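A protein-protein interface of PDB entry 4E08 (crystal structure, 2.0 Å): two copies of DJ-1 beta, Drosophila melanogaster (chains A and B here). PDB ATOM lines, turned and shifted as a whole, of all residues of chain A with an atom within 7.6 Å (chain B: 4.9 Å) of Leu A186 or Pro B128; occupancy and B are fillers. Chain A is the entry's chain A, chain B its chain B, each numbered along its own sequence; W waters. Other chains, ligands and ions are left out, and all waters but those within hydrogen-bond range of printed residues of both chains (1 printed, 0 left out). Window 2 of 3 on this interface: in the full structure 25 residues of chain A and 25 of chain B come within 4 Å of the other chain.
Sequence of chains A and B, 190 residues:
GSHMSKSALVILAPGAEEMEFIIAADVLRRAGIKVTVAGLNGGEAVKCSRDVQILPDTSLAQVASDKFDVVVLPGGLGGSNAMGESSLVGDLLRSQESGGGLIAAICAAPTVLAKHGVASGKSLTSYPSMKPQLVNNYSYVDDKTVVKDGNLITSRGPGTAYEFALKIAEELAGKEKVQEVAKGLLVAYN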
ATOM      1  N   ARG A  30      -0.441 -43.430  26.296  1.00  0.00           N
ATOM      2  CA  ARG A  30      -1.362 -42.643  27.164  1.00  0.00           C
ATOM      3  C   ARG A  30      -2.680 -43.374  27.348  1.00  0.00           C
ATOM      4  O   ARG A  30      -3.266 -43.327  28.420  1.00  0.00           O
ATOM      5  CB  ARG A  30      -1.631 -41.229  26.593  1.00  0.00           C
ATOM      6  CG  ARG A  30      -0.560 -40.204  26.933  1.00  0.00           C
ATOM      7  CD  ARG A  30      -0.657 -38.885  26.119  1.00  0.00           C
ATOM      8  NE  ARG A  30       0.517 -38.058  26.384  1.00  0.00           N
ATOM      9  CZ  ARG A  30       0.521 -36.967  27.147  1.00  0.00           C
ATOM     10  NH1 ARG A  30      -0.610 -36.533  27.696  1.00  0.00           N
ATOM     11  NH2 ARG A  30       1.670 -36.294  27.340  1.00  0.00           N
ATOM     12  N   GLU A 180     -10.762 -39.010  27.860  1.00  0.00           N
ATOM     13  CA  GLU A 180      -9.905 -38.548  28.947  1.00  0.00           C
ATOM     14  C   GLU A 180      -8.485 -38.290  28.431  1.00  0.00           C
ATOM     15  O   GLU A 180      -7.810 -37.365  28.882  1.00  0.00           O
ATOM     16  CB  GLU A 180      -9.808 -39.594  30.044  1.00  0.00           C
ATOM     17  CG  GLU A 180     -11.115 -39.983  30.664  1.00  0.00           C
ATOM     18  CD  GLU A 180     -10.913 -41.048  31.734  1.00  0.00           C
ATOM     19  OE1 GLU A 180      -9.759 -41.516  31.907  1.00  0.00           O
ATOM     20  OE2 GLU A 180     -11.896 -41.441  32.378  1.00  0.00           O
ATOM     21  N   VAL A 181      -8.041 -39.129  27.505  1.00  0.00           N
ATOM     22  CA  VAL A 181      -6.729 -38.970  26.914  1.00  0.00           C
ATOM     23  C   VAL A 181      -6.672 -37.663  26.095  1.00  0.00           C
ATOM     24  O   VAL A 181      -5.791 -36.840  26.324  1.00  0.00           O
ATOM     25  CB  VAL A 181      -6.336 -40.203  26.122  1.00  0.00           C
ATOM     26  CG1 VAL A 181      -5.122 -39.924  25.212  1.00  0.00           C
ATOM     27  CG2 VAL A 181      -6.018 -41.332  27.101  1.00  0.00           C
ATOM     28  N   ALA A 182      -7.651 -37.462  25.215  1.00  0.00           N
ATOM     29  CA  ALA A 182      -7.755 -36.255  24.403  1.00  0.00           C
ATOM     30  C   ALA A 182      -7.866 -34.972  25.246  1.00  0.00           C
ATOM     31  O   ALA A 182      -7.241 -33.936  24.920  1.00  0.00           O
ATOM     32  CB  ALA A 182      -8.920 -36.373  23.465  1.00  0.00           C
ATOM     33  N   LYS A 183      -8.642 -35.041  26.327  1.00  0.00           N
ATOM     34  CA  LYS A 183      -8.773 -33.907  27.253  1.00  0.00           C
ATOM     35  C   LYS A 183      -7.391 -33.523  27.813  1.00  0.00           C
ATOM     36  O   LYS A 183      -7.014 -32.359  27.811  1.00  0.00           O
ATOM     37  CB  LYS A 183      -9.773 -34.241  28.392  1.00  0.00           C
ATOM     38  CG  LYS A 183     -10.116 -33.071  29.335  1.00  0.00           C
ATOM     39  CD  LYS A 183     -10.380 -33.568  30.753  1.00  0.00           C
ATOM     40  CE  LYS A 183     -10.396 -32.430  31.789  1.00  0.00           C
ATOM     41  NZ  LYS A 183      -9.972 -32.896  33.146  1.00  0.00           N
ATOM     42  N   GLY A 184      -6.624 -34.509  28.257  1.00  0.00           N
ATOM     43  CA  GLY A 184      -5.291 -34.277  28.808  1.00  0.00           C
ATOM     44  C   GLY A 184      -4.317 -33.718  27.775  1.00  0.00           C
ATOM     45  O   GLY A 184      -3.442 -32.919  28.117  1.00  0.00           O
ATOM     46  N   LEU A 185      -4.477 -34.131  26.513  1.00  0.00           N
ATOM     47  CA  LEU A 185      -3.694 -33.605  25.364  1.00  0.00           C
ATOM     48  C   LEU A 185      -3.994 -32.162  24.952  1.00  0.00           C
ATOM     49  O   LEU A 185      -3.200 -31.536  24.219  1.00  0.00           O
ATOM     50  CB  LEU A 185      -3.948 -34.502  24.145  1.00  0.00           C
ATOM     51  CG  LEU A 185      -3.414 -35.948  24.179  1.00  0.00           C
ATOM     52  CD1 LEU A 185      -3.895 -36.747  22.990  1.00  0.00           C
ATOM     53  CD2 LEU A 185      -1.900 -35.984  24.278  1.00  0.00           C
ATOM     54  N   LEU A 186      -5.143 -31.649  25.419  1.00  0.00           N
ATOM     55  CA  LEU A 186      -5.777 -30.431  24.900  1.00  0.00           C
ATOM     56  C   LEU A 186      -6.064 -30.566  23.388  1.00  0.00           C
ATOM     57  O   LEU A 186      -5.893 -29.633  22.599  1.00  0.00           O
ATOM     58  CB  LEU A 186      -4.977 -29.173  25.272  1.00  0.00           C
ATOM     59  CG  LEU A 186      -4.286 -29.240  26.654  1.00  0.00           C
ATOM     60  CD1 LEU A 186      -3.192 -28.160  26.811  1.00  0.00           C
ATOM     61  CD2 LEU A 186      -5.326 -29.140  27.827  1.00  0.00           C
ATOM     62  N   VAL A 187      -6.518 -31.754  22.992  1.00  0.00           N
ATOM     63  CA  VAL A 187      -6.923 -32.014  21.609  1.00  0.00           C
ATOM     64  C   VAL A 187      -8.436 -32.204  21.587  1.00  0.00           C
ATOM     65  O   VAL A 187      -8.958 -33.027  22.339  1.00  0.00           O
ATOM     66  CB  VAL A 187      -6.259 -33.287  21.059  1.00  0.00           C
ATOM     67  CG1 VAL A 187      -6.849 -33.693  19.674  1.00  0.00           C
ATOM     68  CG2 VAL A 187      -4.756 -33.122  20.982  1.00  0.00           C
ATOM     69  N   ALA A 188      -9.141 -31.454  20.732  1.00  0.00           N
ATOM     70  CA  ALA A 188     -10.591 -31.658  20.554  1.00  0.00           C
ATOM     71  C   ALA A 188     -10.846 -33.000  19.847  1.00  0.00           C
ATOM     72  O   ALA A 188     -10.290 -33.260  18.789  1.00  0.00           O
ATOM     73  CB  ALA A 188     -11.208 -30.506  19.769  1.00  0.00           C
ATOM     74  N   TYR A 189     -11.641 -33.869  20.464  1.00  0.00           N
ATOM     75  CA  TYR A 189     -11.950 -35.187  19.889  1.00  0.00           C
ATOM     76  C   TYR A 189     -13.232 -35.740  20.495  1.00  0.00           C
ATOM     77  O   TYR A 189     -14.020 -36.343  19.777  1.00  0.00           O
ATOM     78  CB  TYR A 189     -10.811 -36.187  20.132  1.00  0.00           C
ATOM     79  CG  TYR A 189     -10.985 -37.519  19.419  1.00  0.00           C
ATOM     80  CD1 TYR A 189     -10.438 -37.727  18.153  1.00  0.00           C
ATOM     81  CD2 TYR A 189     -11.684 -38.584  20.025  1.00  0.00           C
ATOM     82  CE1 TYR A 189     -10.580 -38.980  17.488  1.00  0.00           C
ATOM     83  CE2 TYR A 189     -11.827 -39.825  19.376  1.00  0.00           C
ATOM     84  CZ  TYR A 189     -11.287 -40.009  18.109  1.00  0.00           C
ATOM     85  OH  TYR A 189     -11.430 -41.220  17.449  1.00  0.00           O
ATOM     86  N   SER B 126       0.317 -21.644  30.049  1.00  0.00           N
ATOM     87  CA  SER B 126       0.995 -22.914  30.366  1.00  0.00           C
ATOM     88  C   SER B 126      -0.009 -24.046  30.254  1.00  0.00           C
ATOM     89  O   SER B 126      -1.168 -23.793  29.957  1.00  0.00           O
ATOM     90  CB  SER B 126       1.506 -22.881  31.787  1.00  0.00           C
ATOM     91  OG  SER B 126       0.408 -22.952  32.661  1.00  0.00           O
ATOM     92  N   TYR B 127       0.403 -25.287  30.533  1.00  0.00           N
ATOM     93  CA  TYR B 127      -0.587 -26.346  30.760  1.00  0.00           C
ATOM     94  C   TYR B 127      -1.582 -25.880  31.862  1.00  0.00           C
ATOM     95  O   TYR B 127      -1.159 -25.408  32.936  1.00  0.00           O
ATOM     96  CB  TYR B 127       0.065 -27.692  31.127  1.00  0.00           C
ATOM     97  CG  TYR B 127      -0.913 -28.819  30.978  1.00  0.00           C
ATOM     98  CD1 TYR B 127      -1.133 -29.389  29.722  1.00  0.00           C
ATOM     99  CD2 TYR B 127      -1.680 -29.260  32.058  1.00  0.00           C
ATOM    100  CE1 TYR B 127      -2.065 -30.396  29.533  1.00  0.00           C
ATOM    101  CE2 TYR B 127      -2.622 -30.298  31.893  1.00  0.00           C
ATOM    102  CZ  TYR B 127      -2.799 -30.860  30.617  1.00  0.00           C
ATOM    103  OH  TYR B 127      -3.711 -31.859  30.395  1.00  0.00           O
ATOM    104  N   PRO B 128      -2.903 -25.987  31.588  1.00  0.00           N
ATOM    105  CA  PRO B 128      -3.961 -25.408  32.408  1.00  0.00           C
ATOM    106  C   PRO B 128      -3.809 -25.766  33.891  1.00  0.00           C
ATOM    107  O   PRO B 128      -4.012 -24.917  34.762  1.00  0.00           O
ATOM    108  CB  PRO B 128      -5.247 -26.044  31.836  1.00  0.00           C
ATOM    109  CG  PRO B 128      -4.949 -26.377  30.510  1.00  0.00           C
ATOM    110  CD  PRO B 128      -3.456 -26.679  30.413  1.00  0.00           C
ATOM    111  N   SER B 129      -3.405 -26.999  34.189  1.00  0.00           N
ATOM    112  CA  SER B 129      -3.377 -27.370  35.614  1.00  0.00           C
ATOM    113  C   SER B 129      -2.146 -26.764  36.312  1.00  0.00           C
ATOM    114  O   SER B 129      -2.087 -26.685  37.539  1.00  0.00           O
ATOM    115  CB  SER B 129      -3.512 -28.879  35.794  1.00  0.00           C
ATOM    116  OG  SER B 129      -2.392 -29.536  35.249  1.00  0.00           O
ATOM    117  N   MET B 130      -1.189 -26.279  35.531  1.00  0.00           N
ATOM    118  CA  MET B 130      -0.024 -25.633  36.131  1.00  0.00           C
ATOM    119  C   MET B 130      -0.264 -24.147  36.508  1.00  0.00           C
ATOM    120  O   MET B 130       0.596 -23.541  37.153  1.00  0.00           O
ATOM    121  CB  MET B 130       1.228 -25.806  35.265  1.00  0.00           C
ATOM    122  CG  MET B 130       1.658 -27.277  35.008  1.00  0.00           C
ATOM    123  SD  MET B 130       1.601 -28.316  36.492  1.00  0.00           S
ATOM    124  CE  MET B 130       2.893 -27.603  37.516  1.00  0.00           C
ATOM    125  N   LYS B 131      -1.426 -23.584  36.136  1.00  0.00           N
ATOM    126  CA  LYS B 131      -1.754 -22.173  36.440  1.00  0.00           C
ATOM    127  C   LYS B 131      -1.357 -21.666  37.862  1.00  0.00           C
ATOM    128  O   LYS B 131      -0.686 -20.625  37.975  1.00  0.00           O
ATOM    129  CB  LYS B 131      -3.228 -21.834  36.109  1.00  0.00           C
ATOM    130  CG  LYS B 131      -3.640 -20.437  36.502  1.00  0.00           C
ATOM    131  CD  LYS B 131      -5.029 -20.103  36.014  1.00  0.00           C
ATOM    132  CE  LYS B 131      -5.435 -18.717  36.465  1.00  0.00           C
ATOM    133  NZ  LYS B 131      -6.678 -18.313  35.751  1.00  0.00           N
ATOM    134  N   PRO B 132      -1.771 -22.381  38.939  1.00  0.00           N
ATOM    135  CA  PRO B 132      -1.412 -21.864  40.271  1.00  0.00           C
ATOM    136  C   PRO B 132       0.071 -21.586  40.536  1.00  0.00           C
ATOM    137  O   PRO B 132       0.370 -20.718  41.353  1.00  0.00           O
ATOM    138  CB  PRO B 132      -1.974 -22.928  41.232  1.00  0.00           C
ATOM    139  CG  PRO B 132      -3.208 -23.438  40.502  1.00  0.00           C
ATOM    140  CD  PRO B 132      -2.740 -23.493  39.035  1.00  0.00           C
ATOM    141  N   TYR B 140      -0.899 -14.203  33.932  1.00  0.00           N
ATOM    142  CA  TYR B 140      -1.344 -15.452  33.334  1.00  0.00           C
ATOM    143  C   TYR B 140      -2.533 -15.206  32.417  1.00  0.00           C
ATOM    144  O   TYR B 140      -3.467 -14.503  32.778  1.00  0.00           O
ATOM    145  CB  TYR B 140      -1.738 -16.458  34.421  1.00  0.00           C
ATOM    146  CG  TYR B 140      -1.869 -17.861  33.887  1.00  0.00           C
ATOM    147  CD1 TYR B 140      -0.764 -18.718  33.855  1.00  0.00           C
ATOM    148  CD2 TYR B 140      -3.090 -18.330  33.393  1.00  0.00           C
ATOM    149  CE1 TYR B 140      -0.860 -20.017  33.335  1.00  0.00           C
ATOM    150  CE2 TYR B 140      -3.206 -19.637  32.877  1.00  0.00           C
ATOM    151  CZ  TYR B 140      -2.093 -20.474  32.859  1.00  0.00           C
ATOM    152  OH  TYR B 140      -2.201 -21.754  32.346  1.00  0.00           O
ATOM    153  N   ARG B 156       0.517 -24.295  25.565  1.00  0.00           N
ATOM    154  CA  ARG B 156      -0.199 -25.047  26.593  1.00  0.00           C
ATOM    155  C   ARG B 156       0.059 -26.553  26.645  1.00  0.00           C
ATOM    156  O   ARG B 156       0.079 -27.139  27.730  1.00  0.00           O
ATOM    157  CB  ARG B 156      -1.720 -24.847  26.433  1.00  0.00           C
ATOM    158  CG  ARG B 156      -2.182 -23.402  26.400  1.00  0.00           C
ATOM    159  CD  ARG B 156      -2.654 -22.931  27.737  1.00  0.00           C
ATOM    160  NE  ARG B 156      -4.071 -23.103  27.817  1.00  0.00           N
ATOM    161  CZ  ARG B 156      -4.831 -22.859  28.873  1.00  0.00           C
ATOM    162  NH1 ARG B 156      -4.331 -22.438  30.047  1.00  0.00           N
ATOM    163  NH2 ARG B 156      -6.129 -23.047  28.720  1.00  0.00           N
ATOM    164  N   GLY B 157       0.167 -27.218  25.499  1.00  0.00           N
ATOM    165  CA  GLY B 157       0.237 -28.668  25.575  1.00  0.00           C
ATOM    166  C   GLY B 157       0.375 -29.302  24.213  1.00  0.00           C
ATOM    167  O   GLY B 157       0.573 -28.587  23.229  1.00  0.00           O
ATOM    168  N   GLY B 159      -1.749 -30.427  22.172  1.00  0.00           N
ATOM    169  CA  GLY B 159      -2.740 -29.905  21.256  1.00  0.00           C
ATOM    170  C   GLY B 159      -2.445 -28.511  20.742  1.00  0.00           C
ATOM    171  O   GLY B 159      -3.110 -28.019  19.832  1.00  0.00           O
HETATM  172  O   HOH W   1      -6.759 -30.661  30.857  1.00  0.00           O
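Water W1 bridges the side-chain hydroxyl of Tyr B127 (3.3 Å) and the backbone carbonyl oxygen of Lys A183 (3.5 Å).
The backbone NH of Tyr B127 sits close to the backbone carbonyl oxygen of Arg B156 (3.4 Å).
O of Ser B126 lies close to NH1 of Arg B156, at 3.4 Å.
The backbone NH (N) of Val A187 lies within hydrogen-bond range of the backbone carbonyl oxygen (O) of Ala A182, 3.0 Å away.
OH of Tyr B140 lies within hydrogen-bond range of NH1 of Arg B156 (3.2 Å).
O of Gly A184 lies within hydrogen-bond range of OH of Tyr B127.
The backbone NH of Gly B159 lies within hydrogen-bond range of the backbone carbonyl oxygen of Leu A185.
Among the printed residues, pairs that only touch across the chains: Leu A186 with Gly B159 (3.4 Å), Leu A186 with Arg B156 (3.5 Å), Leu A186 with Gly B157 (3.7 Å), Leu A186 with Tyr B127 (3.7 Å), Val A187 with Gly B159 (3.8 Å) and Leu A186 with Pro B128 (3.9 Å).
Hydrophobic or aromatic side chains of chain B within 4 Å of the printed part of chain A: Tyr B127 and Pro B128.
Along chain B the printed residues that touch a printed residue of chain A span positions 127 to 159.
Of the 11 printed residues of chain A, 4 touch a printed residue of chain B.
Among the printed residues, no Asp or Glu carboxylate lies within 4 Å of a Lys or Arg side-chain nitrogen of the other chain.
No position is printed for both chains.
Printed residues of chain B within 4 Å of Gly A184: Tyr B127.
Of the printed residues of chain B, Leu A185 touches Gly B159 (2.7 Å).
Printed residues of chain B within 4 Å of Leu A186: Tyr B127, Pro B128, Arg B156, Gly B157 and Gly B159.
Printed residues of chain B within 4 Å of Val A187: Gly B159 (3.8 Å).
Of the printed residues of chain A, Tyr B127 touches Gly A184 (2.5 Å) and Leu A186 (3.7 Å).
Printed residues of chain A within 4 Å of Pro B128: Leu A186.
Ser B129 touches none of the printed residues of chain A.
Printed residues of chain A within 4 Å of Gly B157: Leu A186 (3.7 Å).
The nearest residue of chain A that does not touch Pro B128 is Gly A184 (6.6 Å).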
